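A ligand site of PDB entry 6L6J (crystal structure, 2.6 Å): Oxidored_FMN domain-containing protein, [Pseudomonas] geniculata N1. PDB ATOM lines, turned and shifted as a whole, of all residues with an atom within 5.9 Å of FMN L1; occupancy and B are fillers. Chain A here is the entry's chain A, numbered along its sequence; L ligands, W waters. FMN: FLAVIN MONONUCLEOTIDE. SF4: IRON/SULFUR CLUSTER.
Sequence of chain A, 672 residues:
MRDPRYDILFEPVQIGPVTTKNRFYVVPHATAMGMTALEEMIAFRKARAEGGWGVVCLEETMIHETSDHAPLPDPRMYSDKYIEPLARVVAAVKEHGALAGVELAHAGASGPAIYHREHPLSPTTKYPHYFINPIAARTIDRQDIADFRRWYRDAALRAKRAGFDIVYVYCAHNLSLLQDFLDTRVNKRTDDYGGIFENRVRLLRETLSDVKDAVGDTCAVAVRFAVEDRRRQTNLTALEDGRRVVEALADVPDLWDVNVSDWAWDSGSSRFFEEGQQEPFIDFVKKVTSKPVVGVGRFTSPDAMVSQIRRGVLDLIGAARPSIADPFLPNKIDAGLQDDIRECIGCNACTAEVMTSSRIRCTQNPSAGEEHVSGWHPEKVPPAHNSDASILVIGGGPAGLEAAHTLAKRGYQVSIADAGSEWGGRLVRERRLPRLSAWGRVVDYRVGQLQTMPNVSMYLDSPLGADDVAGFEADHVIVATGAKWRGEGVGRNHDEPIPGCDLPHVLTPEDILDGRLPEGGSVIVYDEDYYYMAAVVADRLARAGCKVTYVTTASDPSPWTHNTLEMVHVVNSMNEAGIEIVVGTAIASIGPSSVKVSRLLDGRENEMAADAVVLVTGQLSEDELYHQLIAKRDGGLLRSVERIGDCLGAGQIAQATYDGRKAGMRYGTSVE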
ATOM      1  N   VAL A  27     -33.497  -2.972  -6.664  1.00  0.00           N
ATOM      2  CA  VAL A  27     -32.814  -3.552  -7.865  1.00  0.00           C
ATOM      3  C   VAL A  27     -31.392  -3.898  -7.469  1.00  0.00           C
ATOM      4  O   VAL A  27     -30.873  -3.358  -6.490  1.00  0.00           O
ATOM      5  CB  VAL A  27     -32.890  -2.608  -9.077  1.00  0.00           C
ATOM      6  CG1 VAL A  27     -34.267  -2.637  -9.695  1.00  0.00           C
ATOM      7  CG2 VAL A  27     -32.492  -1.175  -8.715  1.00  0.00           C
ATOM      8  N   PRO A  28     -30.728  -4.830  -8.188  1.00  0.00           N
ATOM      9  CA  PRO A  28     -29.360  -5.223  -7.855  1.00  0.00           C
ATOM     10  C   PRO A  28     -28.471  -3.981  -7.849  1.00  0.00           C
ATOM     11  O   PRO A  28     -28.488  -3.245  -8.814  1.00  0.00           O
ATOM     12  CB  PRO A  28     -28.916  -6.180  -8.985  1.00  0.00           C
ATOM     13  CG  PRO A  28     -30.170  -6.545  -9.730  1.00  0.00           C
ATOM     14  CD  PRO A  28     -31.250  -5.549  -9.356  1.00  0.00           C
ATOM     15  N   HIS A  29     -27.744  -3.772  -6.766  1.00  0.00           N
ATOM     16  CA  HIS A  29     -26.729  -2.693  -6.649  1.00  0.00           C
ATOM     17  C   HIS A  29     -25.618  -3.167  -5.705  1.00  0.00           C
ATOM     18  O   HIS A  29     -25.965  -3.585  -4.534  1.00  0.00           O
ATOM     19  CB  HIS A  29     -27.396  -1.370  -6.253  1.00  0.00           C
ATOM     20  CG  HIS A  29     -27.509  -1.159  -4.782  1.00  0.00           C
ATOM     21  ND1 HIS A  29     -26.393  -0.897  -4.008  1.00  0.00           N
ATOM     22  CD2 HIS A  29     -28.575  -1.128  -3.951  1.00  0.00           C
ATOM     23  CE1 HIS A  29     -26.769  -0.747  -2.754  1.00  0.00           C
ATOM     24  NE2 HIS A  29     -28.105  -0.860  -2.695  1.00  0.00           N
ATOM     25  N   ALA A  30     -24.376  -3.134  -6.201  1.00  0.00           N
ATOM     26  CA  ALA A  30     -23.157  -3.571  -5.486  1.00  0.00           C
ATOM     27  C   ALA A  30     -22.984  -2.738  -4.235  1.00  0.00           C
ATOM     28  O   ALA A  30     -23.315  -1.546  -4.257  1.00  0.00           O
ATOM     29  CB  ALA A  30     -21.942  -3.459  -6.372  1.00  0.00           C
ATOM     30  N   THR A  31     -22.474  -3.358  -3.169  1.00  0.00           N
ATOM     31  CA  THR A  31     -22.164  -2.690  -1.876  1.00  0.00           C
ATOM     32  C   THR A  31     -20.662  -2.713  -1.598  1.00  0.00           C
ATOM     33  O   THR A  31     -20.258  -2.071  -0.599  1.00  0.00           O
ATOM     34  CB  THR A  31     -22.959  -3.364  -0.741  1.00  0.00           C
ATOM     35  OG1 THR A  31     -22.864  -4.775  -0.979  1.00  0.00           O
ATOM     36  CG2 THR A  31     -24.392  -2.902  -0.699  1.00  0.00           C
ATOM     37  N   GLU A  59     -26.434  -7.944  -5.600  1.00  0.00           N
ATOM     38  CA  GLU A  59     -25.722  -7.333  -6.751  1.00  0.00           C
ATOM     39  C   GLU A  59     -25.164  -8.444  -7.650  1.00  0.00           C
ATOM     40  O   GLU A  59     -25.470  -9.646  -7.399  1.00  0.00           O
ATOM     41  CB  GLU A  59     -24.606  -6.420  -6.233  1.00  0.00           C
ATOM     42  CG  GLU A  59     -23.490  -7.147  -5.489  1.00  0.00           C
ATOM     43  CD  GLU A  59     -23.476  -6.983  -3.966  1.00  0.00           C
ATOM     44  OE1 GLU A  59     -24.565  -7.148  -3.348  1.00  0.00           O
ATOM     45  OE2 GLU A  59     -22.378  -6.724  -3.373  1.00  0.00           O
ATOM     46  N   GLU A  60     -24.363  -8.068  -8.656  1.00  0.00           N
ATOM     47  CA  GLU A  60     -23.761  -9.007  -9.632  1.00  0.00           C
ATOM     48  C   GLU A  60     -23.130 -10.184  -8.867  1.00  0.00           C
ATOM     49  O   GLU A  60     -22.201  -9.956  -8.130  1.00  0.00           O
ATOM     50  CB  GLU A  60     -22.789  -8.305 -10.581  1.00  0.00           C
ATOM     51  CG  GLU A  60     -21.706  -7.466  -9.916  1.00  0.00           C
ATOM     52  CD  GLU A  60     -20.676  -6.970 -10.918  1.00  0.00           C
ATOM     53  OE1 GLU A  60     -21.001  -6.913 -12.157  1.00  0.00           O
ATOM     54  OE2 GLU A  60     -19.548  -6.651 -10.472  1.00  0.00           O
ATOM     55  N   GLU A 103     -28.689 -11.263  -8.596  1.00  0.00           N
ATOM     56  CA  GLU A 103     -28.297 -10.961  -9.979  1.00  0.00           C
ATOM     57  C   GLU A 103     -27.141 -11.893 -10.366  1.00  0.00           C
ATOM     58  O   GLU A 103     -25.995 -11.460 -10.362  1.00  0.00           O
ATOM     59  CB  GLU A 103     -27.971  -9.483 -10.112  1.00  0.00           C
ATOM     60  CG  GLU A 103     -28.028  -8.982 -11.533  1.00  0.00           C
ATOM     61  CD  GLU A 103     -27.486  -7.576 -11.694  1.00  0.00           C
ATOM     62  OE1 GLU A 103     -28.144  -6.798 -12.397  1.00  0.00           O
ATOM     63  OE2 GLU A 103     -26.386  -7.266 -11.123  1.00  0.00           O
ATOM     64  N   TYR A 170     -28.590 -11.935 -16.501  1.00  0.00           N
ATOM     65  CA  TYR A 170     -28.089 -10.528 -16.504  1.00  0.00           C
ATOM     66  C   TYR A 170     -27.548 -10.191 -17.876  1.00  0.00           C
ATOM     67  O   TYR A 170     -26.549 -10.824 -18.325  1.00  0.00           O
ATOM     68  CB  TYR A 170     -27.014 -10.346 -15.449  1.00  0.00           C
ATOM     69  CG  TYR A 170     -26.457  -8.958 -15.352  1.00  0.00           C
ATOM     70  CD1 TYR A 170     -27.270  -7.879 -15.082  1.00  0.00           C
ATOM     71  CD2 TYR A 170     -25.097  -8.720 -15.481  1.00  0.00           C
ATOM     72  CE1 TYR A 170     -26.767  -6.589 -14.968  1.00  0.00           C
ATOM     73  CE2 TYR A 170     -24.576  -7.440 -15.358  1.00  0.00           C
ATOM     74  CZ  TYR A 170     -25.412  -6.378 -15.098  1.00  0.00           C
ATOM     75  OH  TYR A 170     -24.934  -5.112 -14.987  1.00  0.00           O
ATOM     76  N   ALA A 172     -27.009  -6.457 -19.241  1.00  0.00           N
ATOM     77  CA  ALA A 172     -27.114  -5.001 -19.006  1.00  0.00           C
ATOM     78  C   ALA A 172     -25.747  -4.398 -18.693  1.00  0.00           C
ATOM     79  O   ALA A 172     -24.774  -5.143 -18.715  1.00  0.00           O
ATOM     80  CB  ALA A 172     -28.096  -4.728 -17.885  1.00  0.00           C
ATOM     81  N   HIS A 173     -25.705  -3.065 -18.516  1.00  0.00           N
ATOM     82  CA  HIS A 173     -24.551  -2.225 -18.084  1.00  0.00           C
ATOM     83  C   HIS A 173     -23.297  -2.374 -18.967  1.00  0.00           C
ATOM     84  O   HIS A 173     -22.244  -1.802 -18.572  1.00  0.00           O
ATOM     85  CB  HIS A 173     -24.228  -2.549 -16.620  1.00  0.00           C
ATOM     86  CG  HIS A 173     -25.299  -2.085 -15.700  1.00  0.00           C
ATOM     87  ND1 HIS A 173     -26.195  -2.945 -15.122  1.00  0.00           N
ATOM     88  CD2 HIS A 173     -25.641  -0.834 -15.311  1.00  0.00           C
ATOM     89  CE1 HIS A 173     -27.041  -2.244 -14.386  1.00  0.00           C
ATOM     90  NE2 HIS A 173     -26.725  -0.944 -14.480  1.00  0.00           N
ATOM     91  N   ARG A 224     -32.654  -8.858 -16.188  1.00  0.00           N
ATOM     92  CA  ARG A 224     -32.220  -7.445 -16.221  1.00  0.00           C
ATOM     93  C   ARG A 224     -31.720  -7.186 -17.639  1.00  0.00           C
ATOM     94  O   ARG A 224     -30.885  -7.987 -18.119  1.00  0.00           O
ATOM     95  CB  ARG A 224     -31.208  -7.141 -15.126  1.00  0.00           C
ATOM     96  CG  ARG A 224     -30.868  -5.666 -15.043  1.00  0.00           C
ATOM     97  CD  ARG A 224     -31.709  -4.816 -14.117  1.00  0.00           C
ATOM     98  NE  ARG A 224     -30.850  -4.033 -13.236  1.00  0.00           N
ATOM     99  CZ  ARG A 224     -31.100  -2.831 -12.750  1.00  0.00           C
ATOM    100  NH1 ARG A 224     -32.208  -2.187 -13.042  1.00  0.00           N
ATOM    101  NH2 ARG A 224     -30.199  -2.258 -11.974  1.00  0.00           N
ATOM    102  N   ASN A 259     -33.588  -1.094 -17.909  1.00  0.00           N
ATOM    103  CA  ASN A 259     -32.810   0.147 -17.682  1.00  0.00           C
ATOM    104  C   ASN A 259     -32.021   0.498 -18.960  1.00  0.00           C
ATOM    105  O   ASN A 259     -32.231  -0.169 -19.991  1.00  0.00           O
ATOM    106  CB  ASN A 259     -31.932  -0.007 -16.431  1.00  0.00           C
ATOM    107  CG  ASN A 259     -30.788  -0.980 -16.619  1.00  0.00           C
ATOM    108  OD1 ASN A 259     -30.677  -1.640 -17.654  1.00  0.00           O
ATOM    109  ND2 ASN A 259     -29.942  -1.083 -15.600  1.00  0.00           N
ATOM    110  N   TRP A 263     -23.419   2.439 -16.979  1.00  0.00           N
ATOM    111  CA  TRP A 263     -23.701   2.837 -15.583  1.00  0.00           C
ATOM    112  C   TRP A 263     -23.890   4.353 -15.487  1.00  0.00           C
ATOM    113  O   TRP A 263     -24.746   4.782 -14.704  1.00  0.00           O
ATOM    114  CB  TRP A 263     -22.578   2.289 -14.692  1.00  0.00           C
ATOM    115  CG  TRP A 263     -22.920   2.171 -13.242  1.00  0.00           C
ATOM    116  CD1 TRP A 263     -24.112   2.460 -12.633  1.00  0.00           C
ATOM    117  CD2 TRP A 263     -22.044   1.730 -12.185  1.00  0.00           C
ATOM    118  NE1 TRP A 263     -24.018   2.255 -11.270  1.00  0.00           N
ATOM    119  CE2 TRP A 263     -22.754   1.825 -10.977  1.00  0.00           C
ATOM    120  CE3 TRP A 263     -20.709   1.280 -12.161  1.00  0.00           C
ATOM    121  CZ2 TRP A 263     -22.188   1.475  -9.760  1.00  0.00           C
ATOM    122  CZ3 TRP A 263     -20.153   0.932 -10.945  1.00  0.00           C
ATOM    123  CH2 TRP A 263     -20.881   1.030  -9.754  1.00  0.00           C
ATOM    124  N   ASP A 266     -27.306   4.982 -16.484  1.00  0.00           N
ATOM    125  CA  ASP A 266     -28.247   4.231 -15.615  1.00  0.00           C
ATOM    126  C   ASP A 266     -28.348   4.909 -14.231  1.00  0.00           C
ATOM    127  O   ASP A 266     -29.458   5.232 -13.804  1.00  0.00           O
ATOM    128  CB  ASP A 266     -27.821   2.759 -15.490  1.00  0.00           C
ATOM    129  CG  ASP A 266     -28.871   1.857 -14.816  1.00  0.00           C
ATOM    130  OD1 ASP A 266     -30.065   2.142 -14.998  1.00  0.00           O
ATOM    131  OD2 ASP A 266     -28.476   0.880 -14.135  1.00  0.00           O
ATOM    132  N   SER A 267     -27.233   5.063 -13.534  1.00  0.00           N
ATOM    133  CA  SER A 267     -27.158   5.785 -12.249  1.00  0.00           C
ATOM    134  C   SER A 267     -26.794   7.250 -12.541  1.00  0.00           C
ATOM    135  O   SER A 267     -25.709   7.714 -12.082  1.00  0.00           O
ATOM    136  CB  SER A 267     -26.178   5.115 -11.324  1.00  0.00           C
ATOM    137  OG  SER A 267     -26.507   3.745 -11.158  1.00  0.00           O
ATOM    138  N   GLY A 268     -27.658   7.947 -13.289  1.00  0.00           N
ATOM    139  CA  GLY A 268     -27.488   9.342 -13.696  1.00  0.00           C
ATOM    140  C   GLY A 268     -27.404  10.301 -12.508  1.00  0.00           C
ATOM    141  O   GLY A 268     -28.391  10.469 -11.835  1.00  0.00           O
ATOM    142  N   GLN A 278     -35.656   7.732 -17.433  1.00  0.00           N
ATOM    143  CA  GLN A 278     -35.564   6.498 -18.259  1.00  0.00           C
ATOM    144  C   GLN A 278     -36.918   6.205 -18.911  1.00  0.00           C
ATOM    145  O   GLN A 278     -36.969   5.339 -19.811  1.00  0.00           O
ATOM    146  CB  GLN A 278     -35.143   5.277 -17.448  1.00  0.00           C
ATOM    147  CG  GLN A 278     -33.846   5.474 -16.665  1.00  0.00           C
ATOM    148  CD  GLN A 278     -33.124   4.151 -16.442  1.00  0.00           C
ATOM    149  OE1 GLN A 278     -33.624   3.085 -16.795  1.00  0.00           O
ATOM    150  NE2 GLN A 278     -31.944   4.213 -15.842  1.00  0.00           N
ATOM    151  N   VAL A 296     -36.378   1.843 -13.125  1.00  0.00           N
ATOM    152  CA  VAL A 296     -35.725   2.746 -12.137  1.00  0.00           C
ATOM    153  C   VAL A 296     -35.766   4.171 -12.699  1.00  0.00           C
ATOM    154  O   VAL A 296     -35.835   4.327 -13.929  1.00  0.00           O
ATOM    155  CB  VAL A 296     -34.292   2.246 -11.829  1.00  0.00           C
ATOM    156  CG1 VAL A 296     -34.306   0.868 -11.168  1.00  0.00           C
ATOM    157  CG2 VAL A 296     -33.430   2.215 -13.083  1.00  0.00           C
ATOM    158  N   GLY A 297     -35.750   5.166 -11.812  1.00  0.00           N
ATOM    159  CA  GLY A 297     -35.700   6.579 -12.213  1.00  0.00           C
ATOM    160  C   GLY A 297     -35.345   7.484 -11.062  1.00  0.00           C
ATOM    161  O   GLY A 297     -35.877   8.579 -10.957  1.00  0.00           O
ATOM    162  N   ARG A 298     -34.457   7.034 -10.195  1.00  0.00           N
ATOM    163  CA  ARG A 298     -34.121   7.754  -8.943  1.00  0.00           C
ATOM    164  C   ARG A 298     -35.418   8.179  -8.249  1.00  0.00           C
ATOM    165  O   ARG A 298     -35.499   9.340  -7.791  1.00  0.00           O
ATOM    166  CB  ARG A 298     -33.198   8.932  -9.231  1.00  0.00           C
ATOM    167  CG  ARG A 298     -32.193   9.208  -8.122  1.00  0.00           C
ATOM    168  CD  ARG A 298     -31.914  10.680  -7.890  1.00  0.00           C
ATOM    169  NE  ARG A 298     -31.537  11.359  -9.126  1.00  0.00           N
ATOM    170  CZ  ARG A 298     -31.882  12.599  -9.451  1.00  0.00           C
ATOM    171  NH1 ARG A 298     -32.567  13.354  -8.610  1.00  0.00           N
ATOM    172  NH2 ARG A 298     -31.532  13.082 -10.629  1.00  0.00           N
ATOM    173  N   PHE A 299     -36.386   7.263  -8.164  1.00  0.00           N
ATOM    174  CA  PHE A 299     -37.764   7.553  -7.698  1.00  0.00           C
ATOM    175  C   PHE A 299     -37.719   7.942  -6.219  1.00  0.00           C
ATOM    176  O   PHE A 299     -37.197   7.169  -5.412  1.00  0.00           O
ATOM    177  CB  PHE A 299     -38.690   6.386  -8.016  1.00  0.00           C
ATOM    178  CG  PHE A 299     -38.925   6.129  -9.486  1.00  0.00           C
ATOM    179  CD1 PHE A 299     -39.393   7.151 -10.320  1.00  0.00           C
ATOM    180  CD2 PHE A 299     -38.740   4.868 -10.036  1.00  0.00           C
ATOM    181  CE1 PHE A 299     -39.654   6.899 -11.666  1.00  0.00           C
ATOM    182  CE2 PHE A 299     -39.009   4.625 -11.376  1.00  0.00           C
ATOM    183  CZ  PHE A 299     -39.463   5.636 -12.186  1.00  0.00           C
ATOM    184  N   GLY A 318     -38.870   0.317  -9.303  1.00  0.00           N
ATOM    185  CA  GLY A 318     -37.465  -0.083  -9.108  1.00  0.00           C
ATOM    186  C   GLY A 318     -36.678   1.025  -8.435  1.00  0.00           C
ATOM    187  O   GLY A 318     -36.822   2.174  -8.868  1.00  0.00           O
ATOM    188  N   ALA A 319     -35.868   0.684  -7.430  1.00  0.00           N
ATOM    189  CA  ALA A 319     -34.964   1.653  -6.769  1.00  0.00           C
ATOM    190  C   ALA A 319     -33.647   1.003  -6.358  1.00  0.00           C
ATOM    191  O   ALA A 319     -33.657  -0.158  -5.944  1.00  0.00           O
ATOM    192  CB  ALA A 319     -35.644   2.290  -5.583  1.00  0.00           C
ATOM    193  N   ALA A 320     -32.562   1.752  -6.497  1.00  0.00           N
ATOM    194  CA  ALA A 320     -31.263   1.479  -5.825  1.00  0.00           C
ATOM    195  C   ALA A 320     -30.963   2.677  -4.908  1.00  0.00           C
ATOM    196  O   ALA A 320     -31.135   2.534  -3.701  1.00  0.00           O
ATOM    197  CB  ALA A 320     -30.159   1.217  -6.838  1.00  0.00           C
ATOM    198  N   ARG A 321     -30.588   3.808  -5.491  1.00  0.00           N
ATOM    199  CA  ARG A 321     -30.077   4.986  -4.725  1.00  0.00           C
ATOM    200  C   ARG A 321     -31.107   5.421  -3.692  1.00  0.00           C
ATOM    201  O   ARG A 321     -30.782   5.624  -2.531  1.00  0.00           O
ATOM    202  CB  ARG A 321     -29.636   6.127  -5.649  1.00  0.00           C
ATOM    203  CG  ARG A 321     -28.207   5.964  -6.147  1.00  0.00           C
ATOM    204  CD  ARG A 321     -27.809   6.869  -7.271  1.00  0.00           C
ATOM    205  NE  ARG A 321     -28.769   6.815  -8.378  1.00  0.00           N
ATOM    206  CZ  ARG A 321     -28.776   7.672  -9.380  1.00  0.00           C
ATOM    207  NH1 ARG A 321     -27.863   8.628  -9.459  1.00  0.00           N
ATOM    208  NH2 ARG A 321     -29.703   7.596 -10.298  1.00  0.00           N
ATOM    209  N   PRO A 322     -32.394   5.588  -4.061  1.00  0.00           N
ATOM    210  CA  PRO A 322     -33.407   5.976  -3.082  1.00  0.00           C
ATOM    211  C   PRO A 322     -33.473   5.039  -1.866  1.00  0.00           C
ATOM    212  O   PRO A 322     -33.588   5.541  -0.729  1.00  0.00           O
ATOM    213  CB  PRO A 322     -34.715   5.962  -3.891  1.00  0.00           C
ATOM    214  CG  PRO A 322     -34.230   6.253  -5.298  1.00  0.00           C
ATOM    215  CD  PRO A 322     -32.925   5.506  -5.429  1.00  0.00           C
ATOM    216  N   ILE A 324     -30.940   3.397  -0.709  1.00  0.00           N
ATOM    217  CA  ILE A 324     -29.636   3.571  -0.017  1.00  0.00           C
ATOM    218  C   ILE A 324     -29.805   4.726   0.965  1.00  0.00           C
ATOM    219  O   ILE A 324     -29.476   4.561   2.156  1.00  0.00           O
ATOM    220  CB  ILE A 324     -28.492   3.813  -1.028  1.00  0.00           C
ATOM    221  CG1 ILE A 324     -28.100   2.511  -1.737  1.00  0.00           C
ATOM    222  CG2 ILE A 324     -27.280   4.475  -0.366  1.00  0.00           C
ATOM    223  CD1 ILE A 324     -27.165   2.710  -2.945  1.00  0.00           C
ATOM    224  N   ASN A 348     -23.809  10.624  -6.307  1.00  0.00           N
ATOM    225  CA  ASN A 348     -23.117   9.361  -6.723  1.00  0.00           C
ATOM    226  C   ASN A 348     -21.843   9.122  -5.884  1.00  0.00           C
ATOM    227  O   ASN A 348     -20.921   8.440  -6.377  1.00  0.00           O
ATOM    228  CB  ASN A 348     -22.837   9.354  -8.213  1.00  0.00           C
ATOM    229  CG  ASN A 348     -24.035   8.950  -9.051  1.00  0.00           C
ATOM    230  OD1 ASN A 348     -25.132   8.744  -8.519  1.00  0.00           O
ATOM    231  ND2 ASN A 348     -23.851   8.832 -10.366  1.00  0.00           N
ATOM    232  N   CYS A 350     -22.000   7.115  -3.404  1.00  0.00           N
ATOM    233  CA  CYS A 350     -22.206   5.634  -3.249  1.00  0.00           C
ATOM    234  C   CYS A 350     -21.482   4.894  -4.378  1.00  0.00           C
ATOM    235  O   CYS A 350     -20.718   3.945  -4.136  1.00  0.00           O
ATOM    236  CB  CYS A 350     -23.697   5.279  -3.247  1.00  0.00           C
ATOM    237  SG  CYS A 350     -24.690   6.069  -4.533  1.00  0.00           S
ATOM    238  N   THR A 351     -21.705   5.363  -5.598  1.00  0.00           N
ATOM    239  CA  THR A 351     -21.045   4.932  -6.862  1.00  0.00           C
ATOM    240  C   THR A 351     -19.518   5.056  -6.705  1.00  0.00           C
ATOM    241  O   THR A 351     -18.769   4.113  -7.149  1.00  0.00           O
ATOM    242  CB  THR A 351     -21.700   5.769  -7.978  1.00  0.00           C
ATOM    243  OG1 THR A 351     -22.988   5.164  -8.196  1.00  0.00           O
ATOM    244  CG2 THR A 351     -20.916   5.840  -9.259  1.00  0.00           C
ATOM    245  N   VAL A 354     -17.789   2.447  -4.486  1.00  0.00           N
ATOM    246  CA  VAL A 354     -17.954   1.141  -5.192  1.00  0.00           C
ATOM    247  C   VAL A 354     -16.996   1.105  -6.391  1.00  0.00           C
ATOM    248  O   VAL A 354     -16.390   0.031  -6.637  1.00  0.00           O
ATOM    249  CB  VAL A 354     -19.413   0.853  -5.572  1.00  0.00           C
ATOM    250  CG1 VAL A 354     -19.547  -0.400  -6.432  1.00  0.00           C
ATOM    251  CG2 VAL A 354     -20.272   0.747  -4.322  1.00  0.00           C
ATOM    252  N   ILE A 360     -19.439   0.732   0.413  1.00  0.00           N
ATOM    253  CA  ILE A 360     -20.413   1.796  -0.014  1.00  0.00           C
ATOM    254  C   ILE A 360     -20.646   2.790   1.134  1.00  0.00           C
ATOM    255  O   ILE A 360     -20.565   2.394   2.292  1.00  0.00           O
ATOM    256  CB  ILE A 360     -21.725   1.154  -0.504  1.00  0.00           C
ATOM    257  CG1 ILE A 360     -22.707   2.191  -1.074  1.00  0.00           C
ATOM    258  CG2 ILE A 360     -22.381   0.344   0.615  1.00  0.00           C
ATOM    259  CD1 ILE A 360     -23.888   1.589  -1.798  1.00  0.00           C
HETATM  260  N1  FMN L   1     -26.840  -2.478 -11.328  1.00  0.00           N
HETATM  261  C2  FMN L   1     -26.591  -3.796 -11.584  1.00  0.00           C
HETATM  262  O2  FMN L   1     -27.259  -4.343 -12.460  1.00  0.00           O
HETATM  263  N3  FMN L   1     -25.709  -4.554 -10.918  1.00  0.00           N
HETATM  264  C4  FMN L   1     -24.970  -4.030  -9.911  1.00  0.00           C
HETATM  265  O4  FMN L   1     -24.159  -4.723  -9.305  1.00  0.00           O
HETATM  266  C4A FMN L   1     -25.151  -2.588  -9.585  1.00  0.00           C
HETATM  267  N5  FMN L   1     -24.438  -2.000  -8.598  1.00  0.00           N
HETATM  268  C5A FMN L   1     -24.680  -0.705  -8.276  1.00  0.00           C
HETATM  269  C6  FMN L   1     -24.007  -0.117  -7.215  1.00  0.00           C
HETATM  270  C7  FMN L   1     -24.286   1.193  -6.892  1.00  0.00           C
HETATM  271  C7M FMN L   1     -23.506   1.825  -5.797  1.00  0.00           C
HETATM  272  C8  FMN L   1     -25.303   1.957  -7.624  1.00  0.00           C
HETATM  273  C8M FMN L   1     -25.587   3.398  -7.304  1.00  0.00           C
HETATM  274  C9  FMN L   1     -25.972   1.397  -8.671  1.00  0.00           C
HETATM  275  C9A FMN L   1     -25.731   0.080  -9.028  1.00  0.00           C
HETATM  276  N10 FMN L   1     -26.442  -0.536 -10.072  1.00  0.00           N
HETATM  277  C10 FMN L   1     -26.168  -1.846 -10.353  1.00  0.00           C
HETATM  278  C1' FMN L   1     -27.490   0.191 -10.864  1.00  0.00           C
HETATM  279  C2' FMN L   1     -28.805   0.215 -10.107  1.00  0.00           C
HETATM  280  O2' FMN L   1     -29.269  -1.120 -10.037  1.00  0.00           O
HETATM  281  C3' FMN L   1     -29.846   1.056 -10.773  1.00  0.00           C
HETATM  282  O3' FMN L   1     -30.186   0.466 -12.028  1.00  0.00           O
HETATM  283  C4' FMN L   1     -29.441   2.511 -10.988  1.00  0.00           C
HETATM  284  O4' FMN L   1     -28.789   3.024  -9.807  1.00  0.00           O
HETATM  285  C5' FMN L   1     -30.635   3.375 -11.381  1.00  0.00           C
HETATM  286  O5' FMN L   1     -31.570   3.342 -10.312  1.00  0.00           O
HETATM  287  P   FMN L   1     -31.571   4.506  -9.182  1.00  0.00           P
HETATM  288  O1P FMN L   1     -31.908   5.782  -9.912  1.00  0.00           O
HETATM  289  O2P FMN L   1     -32.630   4.023  -8.248  1.00  0.00           O
HETATM  290  O3P FMN L   1     -30.179   4.489  -8.590  1.00  0.00           O
HETATM  291 FE1  SF4 L   2     -25.728  10.615  -2.959  1.00  0.00          FE
HETATM  292 FE2  SF4 L   2     -28.332   9.122  -3.377  1.00  0.00          FE
HETATM  293 FE3  SF4 L   2     -26.701   8.667  -0.915  1.00  0.00          FE
HETATM  294 FE4  SF4 L   2     -25.766   7.595  -3.585  1.00  0.00          FE
HETATM  295  S1  SF4 L   2     -27.501   7.407  -2.455  1.00  0.00           S
HETATM  296  S2  SF4 L   2     -24.927   8.869  -2.090  1.00  0.00           S
HETATM  297  S3  SF4 L   2     -26.531   9.333  -4.506  1.00  0.00           S
HETATM  298  S4  SF4 L   2     -27.509  10.349  -1.833  1.00  0.00           S
HETATM  299  O   HOH W   1     -35.234   4.524  -9.206  1.00  0.00           O
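NE2 of His 173 sits close to ND2 of Asn 259 (3.4 Å).
The backbone NH of Val 27 is in hydrogen-bond range of the backbone carbonyl oxygen of Ala 319, 2.9 Å away.
N of Glu 60 is in hydrogen-bond range of OE2 of Glu 103 (3.3 Å).
The side-chain carboxylate of Asp 266 lies within hydrogen-bond range of the side-chain amide nitrogen of Gln 278, 2.9 Å away.
The side-chain carboxylate of Asp 266 lies within hydrogen-bond range of a ring nitrogen (NE2) of His 173 (2.6 Å).
The side-chain amide nitrogen (ND2) of Asn 259 sits at hydrogen-bond distance from the side-chain carboxylate (OD2) of Asp 266, 2.9 Å away.
The side-chain hydroxyl of Thr 31 lies within hydrogen-bond range of the side-chain carboxylate of Glu 59.
O of Ser 267 sits at hydrogen-bond distance from ND2 of Asn 348 (2.8 Å).
Val 27 touches FMN L1.
CA of His 29 touches N5 of FMN L1 (3.1 Å).
Glu 59 touches FMN L1 (CB to O4, 3.5 Å).
Tyr 170 touches FMN L1.
Asn 259 touches FMN L1.
Trp 263 touches FMN L1 (NE1 to C9, 3.4 Å).
Val 296 touches FMN L1 (CB to O5', 3.3 Å).
Ala 319 touches FMN L1.
Pro 322 touches FMN L1.
O of Cys 350 touches C7M of FMN L1 (3.9 Å).
Thr 351 touches FMN L1.
Val 354 touches FMN L1.
Hydrophobic or aromatic side chains within 4 Å of FMN L1: Val 27, His 29, Ala 30, Tyr 170, His 173, Trp 263, Val 296, Ala 320, Pro 322 and Val 354.
Of the 33 residues printed, 23 come within 4 Å of FMN L1.
O3' of FMN L1 lies within hydrogen-bond range of OD2 of Asp 266 (2.7 Å).
N of Arg 298 is in hydrogen-bond range of O1P of FMN L1 (2.9 Å).
The guanidinium group of Arg 224 lies within hydrogen-bond range of an oxygen (O2') of FMN L1, at 2.4 Å.
N of Asn 348 sits close to S3 of SF4 L2, 3.5 Å away.
O2' of FMN L1 sits at hydrogen-bond distance from O of Pro 28 (2.6 Å).
An iron atom (FE4) of SF4 L2 is bound by the side-chain sulfur of Cys 350 (2.1 Å).
ND1 of His 173 sits close to O2 of FMN L1.
A nitrogen (N3) of FMN L1 is in hydrogen-bond range of the side-chain carboxylate of Glu 103 (2.8 Å).
O2P of FMN L1 lies within hydrogen-bond range of N of Ala 320 (2.9 Å).
O3P of FMN L1 is in hydrogen-bond range of N of Arg 321.
OG of Ser 267 sits at hydrogen-bond distance from O4' of FMN L1.
The backbone NH (N) of Ala 30 is in hydrogen-bond range of a nitrogen (N5) of FMN L1 (2.7 Å).
S2 of SF4 L2 sits close to N of Cys 350 (3.7 Å).
NE of Arg 321 is in salt-bridge range of O3P of FMN L1 (2.7 Å).
N of Glu 60 is in hydrogen-bond range of O4 of FMN L1.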
